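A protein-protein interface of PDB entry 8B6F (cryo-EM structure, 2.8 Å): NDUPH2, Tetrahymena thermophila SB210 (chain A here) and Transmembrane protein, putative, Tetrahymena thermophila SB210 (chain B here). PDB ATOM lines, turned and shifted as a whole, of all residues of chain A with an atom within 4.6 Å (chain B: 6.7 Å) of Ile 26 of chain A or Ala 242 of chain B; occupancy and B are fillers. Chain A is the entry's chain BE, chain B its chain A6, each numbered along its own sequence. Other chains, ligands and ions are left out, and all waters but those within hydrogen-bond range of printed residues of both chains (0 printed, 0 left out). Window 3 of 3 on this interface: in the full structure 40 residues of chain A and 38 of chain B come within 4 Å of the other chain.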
ATOM      1  N   TYR A  24      10.424 -15.975 -33.521  1.00  0.00           N
ATOM      2  CA  TYR A  24      10.885 -15.805 -32.152  1.00  0.00           C
ATOM      3  C   TYR A  24      12.395 -15.964 -32.084  1.00  0.00           C
ATOM      4  O   TYR A  24      12.971 -16.817 -32.765  1.00  0.00           O
ATOM      5  CB  TYR A  24      10.213 -16.816 -31.225  1.00  0.00           C
ATOM      6  CG  TYR A  24       8.710 -16.712 -31.225  1.00  0.00           C
ATOM      7  CD1 TYR A  24       8.052 -15.869 -30.340  1.00  0.00           C
ATOM      8  CD2 TYR A  24       7.949 -17.448 -32.118  1.00  0.00           C
ATOM      9  CE1 TYR A  24       6.678 -15.770 -30.343  1.00  0.00           C
ATOM     10  CE2 TYR A  24       6.578 -17.357 -32.128  1.00  0.00           C
ATOM     11  CZ  TYR A  24       5.949 -16.515 -31.241  1.00  0.00           C
ATOM     12  OH  TYR A  24       4.582 -16.434 -31.260  1.00  0.00           O
ATOM     13  N   ASN A  25      13.032 -15.133 -31.260  1.00  0.00           N
ATOM     14  CA  ASN A  25      14.488 -15.120 -31.136  1.00  0.00           C
ATOM     15  C   ASN A  25      14.904 -16.176 -30.116  1.00  0.00           C
ATOM     16  O   ASN A  25      15.124 -15.901 -28.935  1.00  0.00           O
ATOM     17  CB  ASN A  25      14.977 -13.732 -30.742  1.00  0.00           C
ATOM     18  CG  ASN A  25      14.474 -12.652 -31.675  1.00  0.00           C
ATOM     19  OD1 ASN A  25      13.435 -12.803 -32.314  1.00  0.00           O
ATOM     20  ND2 ASN A  25      15.215 -11.556 -31.763  1.00  0.00           N
ATOM     21  N   ILE A  26      15.010 -17.412 -30.590  1.00  0.00           N
ATOM     22  CA  ILE A  26      15.458 -18.527 -29.766  1.00  0.00           C
ATOM     23  C   ILE A  26      16.960 -18.688 -29.950  1.00  0.00           C
ATOM     24  O   ILE A  26      17.452 -18.767 -31.082  1.00  0.00           O
ATOM     25  CB  ILE A  26      14.710 -19.819 -30.132  1.00  0.00           C
ATOM     26  CG1 ILE A  26      13.200 -19.611 -29.976  1.00  0.00           C
ATOM     27  CG2 ILE A  26      15.191 -20.976 -29.263  1.00  0.00           C
ATOM     28  CD1 ILE A  26      12.357 -20.806 -30.376  1.00  0.00           C
ATOM     29  N   MET A  27      17.689 -18.741 -28.840  1.00  0.00           N
ATOM     30  CA  MET A  27      19.144 -18.795 -28.854  1.00  0.00           C
ATOM     31  C   MET A  27      19.619 -20.236 -28.725  1.00  0.00           C
ATOM     32  O   MET A  27      19.025 -21.034 -27.995  1.00  0.00           O
ATOM     33  CB  MET A  27      19.720 -17.946 -27.721  1.00  0.00           C
ATOM     34  CG  MET A  27      19.347 -16.473 -27.827  1.00  0.00           C
ATOM     35  SD  MET A  27      19.891 -15.482 -26.424  1.00  0.00           S
ATOM     36  CE  MET A  27      18.872 -16.150 -25.114  1.00  0.00           C
ATOM     37  N   ARG A  28      20.698 -20.561 -29.437  1.00  0.00           N
ATOM     38  CA  ARG A  28      21.186 -21.930 -29.543  1.00  0.00           C
ATOM     39  C   ARG A  28      22.495 -22.173 -28.803  1.00  0.00           C
ATOM     40  O   ARG A  28      22.965 -23.315 -28.770  1.00  0.00           O
ATOM     41  CB  ARG A  28      21.351 -22.314 -31.019  1.00  0.00           C
ATOM     42  CG  ARG A  28      22.063 -21.270 -31.871  1.00  0.00           C
ATOM     43  CD  ARG A  28      22.106 -21.693 -33.330  1.00  0.00           C
ATOM     44  NE  ARG A  28      23.089 -22.744 -33.570  1.00  0.00           N
ATOM     45  CZ  ARG A  28      24.329 -22.540 -33.993  1.00  0.00           C
ATOM     46  NH1 ARG A  28      24.786 -21.324 -34.244  1.00  0.00           N
ATOM     47  NH2 ARG A  28      25.132 -23.584 -34.174  1.00  0.00           N
ATOM     48  N   ASP B  89      25.107 -13.656 -30.302  1.00  0.00           N
ATOM     49  CA  ASP B  89      23.677 -13.900 -30.441  1.00  0.00           C
ATOM     50  C   ASP B  89      23.109 -14.732 -29.301  1.00  0.00           C
ATOM     51  O   ASP B  89      21.895 -14.963 -29.271  1.00  0.00           O
ATOM     52  CB  ASP B  89      23.384 -14.596 -31.772  1.00  0.00           C
ATOM     53  CG  ASP B  89      23.596 -13.686 -32.966  1.00  0.00           C
ATOM     54  OD1 ASP B  89      24.047 -12.539 -32.768  1.00  0.00           O
ATOM     55  OD2 ASP B  89      23.305 -14.116 -34.101  1.00  0.00           O
ATOM     56  N   VAL B 103      14.462 -18.024 -18.961  1.00  0.00           N
ATOM     57  CA  VAL B 103      13.771 -18.516 -20.149  1.00  0.00           C
ATOM     58  C   VAL B 103      13.601 -17.386 -21.156  1.00  0.00           C
ATOM     59  O   VAL B 103      13.961 -17.528 -22.329  1.00  0.00           O
ATOM     60  CB  VAL B 103      12.409 -19.129 -19.776  1.00  0.00           C
ATOM     61  CG1 VAL B 103      11.662 -19.587 -21.021  1.00  0.00           C
ATOM     62  CG2 VAL B 103      12.594 -20.284 -18.809  1.00  0.00           C
ATOM     63  N   GLY B 238      12.068 -10.191 -28.359  1.00  0.00           N
ATOM     64  CA  GLY B 238      12.612 -10.685 -27.110  1.00  0.00           C
ATOM     65  C   GLY B 238      13.334 -11.999 -27.328  1.00  0.00           C
ATOM     66  O   GLY B 238      13.001 -12.765 -28.234  1.00  0.00           O
ATOM     67  N   VAL B 239      14.328 -12.256 -26.487  1.00  0.00           N
ATOM     68  CA  VAL B 239      15.175 -13.435 -26.621  1.00  0.00           C
ATOM     69  C   VAL B 239      14.606 -14.558 -25.764  1.00  0.00           C
ATOM     70  O   VAL B 239      14.276 -14.352 -24.590  1.00  0.00           O
ATOM     71  CB  VAL B 239      16.628 -13.117 -26.229  1.00  0.00           C
ATOM     72  CG1 VAL B 239      17.171 -11.992 -27.091  1.00  0.00           C
ATOM     73  CG2 VAL B 239      16.736 -12.751 -24.754  1.00  0.00           C
ATOM     74  N   TRP B 240      14.477 -15.740 -26.356  1.00  0.00           N
ATOM     75  CA  TRP B 240      14.059 -16.942 -25.655  1.00  0.00           C
ATOM     76  C   TRP B 240      15.218 -17.927 -25.610  1.00  0.00           C
ATOM     77  O   TRP B 240      16.080 -17.937 -26.493  1.00  0.00           O
ATOM     78  CB  TRP B 240      12.853 -17.597 -26.335  1.00  0.00           C
ATOM     79  CG  TRP B 240      11.592 -16.805 -26.229  1.00  0.00           C
ATOM     80  CD1 TRP B 240      11.202 -15.776 -27.034  1.00  0.00           C
ATOM     81  CD2 TRP B 240      10.551 -16.975 -25.262  1.00  0.00           C
ATOM     82  NE1 TRP B 240       9.982 -15.295 -26.628  1.00  0.00           N
ATOM     83  CE2 TRP B 240       9.561 -16.014 -25.540  1.00  0.00           C
ATOM     84  CE3 TRP B 240      10.361 -17.847 -24.186  1.00  0.00           C
ATOM     85  CZ2 TRP B 240       8.398 -15.901 -24.784  1.00  0.00           C
ATOM     86  CZ3 TRP B 240       9.206 -17.734 -23.435  1.00  0.00           C
ATOM     87  CH2 TRP B 240       8.238 -16.767 -23.737  1.00  0.00           C
ATOM     88  N   ASP B 241      15.236 -18.753 -24.570  1.00  0.00           N
ATOM     89  CA  ASP B 241      16.275 -19.755 -24.385  1.00  0.00           C
ATOM     90  C   ASP B 241      15.748 -21.119 -24.802  1.00  0.00           C
ATOM     91  O   ASP B 241      14.711 -21.568 -24.306  1.00  0.00           O
ATOM     92  CB  ASP B 241      16.743 -19.788 -22.929  1.00  0.00           C
ATOM     93  CG  ASP B 241      17.880 -20.764 -22.706  1.00  0.00           C
ATOM     94  OD1 ASP B 241      18.957 -20.574 -23.309  1.00  0.00           O
ATOM     95  OD2 ASP B 241      17.698 -21.720 -21.925  1.00  0.00           O
ATOM     96  N   ALA B 242      16.466 -21.775 -25.717  1.00  0.00           N
ATOM     97  CA  ALA B 242      16.043 -23.093 -26.178  1.00  0.00           C
ATOM     98  C   ALA B 242      16.019 -24.093 -25.031  1.00  0.00           C
ATOM     99  O   ALA B 242      15.067 -24.868 -24.891  1.00  0.00           O
ATOM    100  CB  ALA B 242      16.969 -23.579 -27.291  1.00  0.00           C
ATOM    101  N   LYS B 243      17.064 -24.093 -24.200  1.00  0.00           N
ATOM    102  CA  LYS B 243      17.104 -25.009 -23.066  1.00  0.00           C
ATOM    103  C   LYS B 243      15.969 -24.721 -22.090  1.00  0.00           C
ATOM    104  O   LYS B 243      15.322 -25.647 -21.587  1.00  0.00           O
ATOM    105  CB  LYS B 243      18.456 -24.910 -22.364  1.00  0.00           C
ATOM    106  CG  LYS B 243      18.632 -25.900 -21.221  1.00  0.00           C
ATOM    107  CD  LYS B 243      19.953 -25.695 -20.492  1.00  0.00           C
ATOM    108  CE  LYS B 243      21.151 -25.914 -21.406  1.00  0.00           C
ATOM    109  NZ  LYS B 243      21.116 -27.241 -22.083  1.00  0.00           N
ATOM    110  N   GLY B 244      15.712 -23.443 -21.810  1.00  0.00           N
ATOM    111  CA  GLY B 244      14.623 -23.101 -20.910  1.00  0.00           C
ATOM    112  C   GLY B 244      13.272 -23.544 -21.437  1.00  0.00           C
ATOM    113  O   GLY B 244      12.436 -24.047 -20.684  1.00  0.00           O
ATOM    114  N   LEU B 245      13.041 -23.366 -22.738  1.00  0.00           N
ATOM    115  CA  LEU B 245      11.783 -23.807 -23.332  1.00  0.00           C
ATOM    116  C   LEU B 245      11.660 -25.324 -23.305  1.00  0.00           C
ATOM    117  O   LEU B 245      10.566 -25.860 -23.090  1.00  0.00           O
ATOM    118  CB  LEU B 245      11.670 -23.287 -24.764  1.00  0.00           C
ATOM    119  CG  LEU B 245      11.435 -21.784 -24.924  1.00  0.00           C
ATOM    120  CD1 LEU B 245      11.493 -21.391 -26.389  1.00  0.00           C
ATOM    121  CD2 LEU B 245      10.099 -21.381 -24.321  1.00  0.00           C
ATOM    122  N   ASN B 246      12.765 -26.034 -23.523  1.00  0.00           N
ATOM    123  CA  ASN B 246      12.741 -27.489 -23.585  1.00  0.00           C
ATOM    124  C   ASN B 246      12.835 -28.149 -22.217  1.00  0.00           C
ATOM    125  O   ASN B 246      12.764 -29.380 -22.139  1.00  0.00           O
ATOM    126  CB  ASN B 246      13.883 -27.991 -24.471  1.00  0.00           C
ATOM    127  CG  ASN B 246      13.825 -27.421 -25.870  1.00  0.00           C
ATOM    128  OD1 ASN B 246      13.188 -26.397 -26.108  1.00  0.00           O
ATOM    129  ND2 ASN B 246      14.490 -28.086 -26.807  1.00  0.00           N
ATOM    130  N   HIS B 247      12.994 -27.380 -21.147  1.00  0.00           N
ATOM    131  CA  HIS B 247      13.056 -27.977 -19.822  1.00  0.00           C
ATOM    132  C   HIS B 247      11.755 -28.726 -19.535  1.00  0.00           C
ATOM    133  O   HIS B 247      10.671 -28.229 -19.856  1.00  0.00           O
ATOM    134  CB  HIS B 247      13.287 -26.900 -18.761  1.00  0.00           C
ATOM    135  CG  HIS B 247      13.752 -27.441 -17.446  1.00  0.00           C
ATOM    136  ND1 HIS B 247      15.057 -27.826 -17.220  1.00  0.00           N
ATOM    137  CD2 HIS B 247      13.088 -27.671 -16.290  1.00  0.00           C
ATOM    138  CE1 HIS B 247      15.176 -28.264 -15.980  1.00  0.00           C
ATOM    139  NE2 HIS B 247      13.996 -28.181 -15.394  1.00  0.00           N
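Of chain B, only Trp 240 (3.4 Å) and Ala 242 (3.7 Å) come within 4 Å of Ile 26 of chain A. Ala 242 of chain B touches just these residues of chain A: Ile 26 (3.7 Å) and Met 27 (3.3 Å). Printed residues of chain A within 4 Å of Trp 240 of chain B: Asn 25, Ile 26 and Met 27. Of the printed residues of chain A, Asp 89 of chain B touches Met 27. Of the printed residues of chain B, Met 27 of chain A touches Asp 89 (3.3 Å), Val 239 (3.9 Å), Trp 240 (3.0 Å) and Ala 242 (3.3 Å). Arg 28 of chain A touches none of the printed residues of chain B. Tyr 24 of chain A touches none of the printed residues of chain B. The nearest printed residue of chain A that does not touch Ala 242 of chain B is Arg 28 of chain A (5.1 Å). The nearest printed residue of chain B that does not touch Asn 25 of chain A is Asp 241 of chain B (5.2 Å).
OD1 of Asn 246 of chain B sits close to O of Ala 242 of chain B (2.7 Å).
Of the 12 printed residues of chain B, 5 touch a printed residue of chain A. Hydrophobic or aromatic side chains of chain B within 4 Å of the printed part of chain A: Val 239, Trp 240 and Ala 242.
The side-chain sulfur of Met 27 of chain A sits close to the backbone carbonyl oxygen of Asp 89 of chain B (3.5 Å). The backbone NH (N) of Met 27 of chain A sits at hydrogen-bond distance from the backbone carbonyl oxygen (O) of Trp 240 of chain B, 3.0 Å away. The backbone NH (N) of Trp 240 of chain B sits at hydrogen-bond distance from the backbone carbonyl oxygen (O) of Asn 25 of chain A, at 2.7 Å.
Asn 25 of chain A touches Gly 238 of chain B. O of Asn 25 of chain A touches CA of Val 239 of chain B (3.4 Å). Trp 240 of chain B touches Ile 26 of chain A. CB of Ala 242 of chain B touches CG2 of Ile 26 of chain A, at 3.7 Å. CE of Met 27 of chain A touches CB of Val 239 of chain B, 3.9 Å away. Met 27 of chain A touches Ala 242 of chain B.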
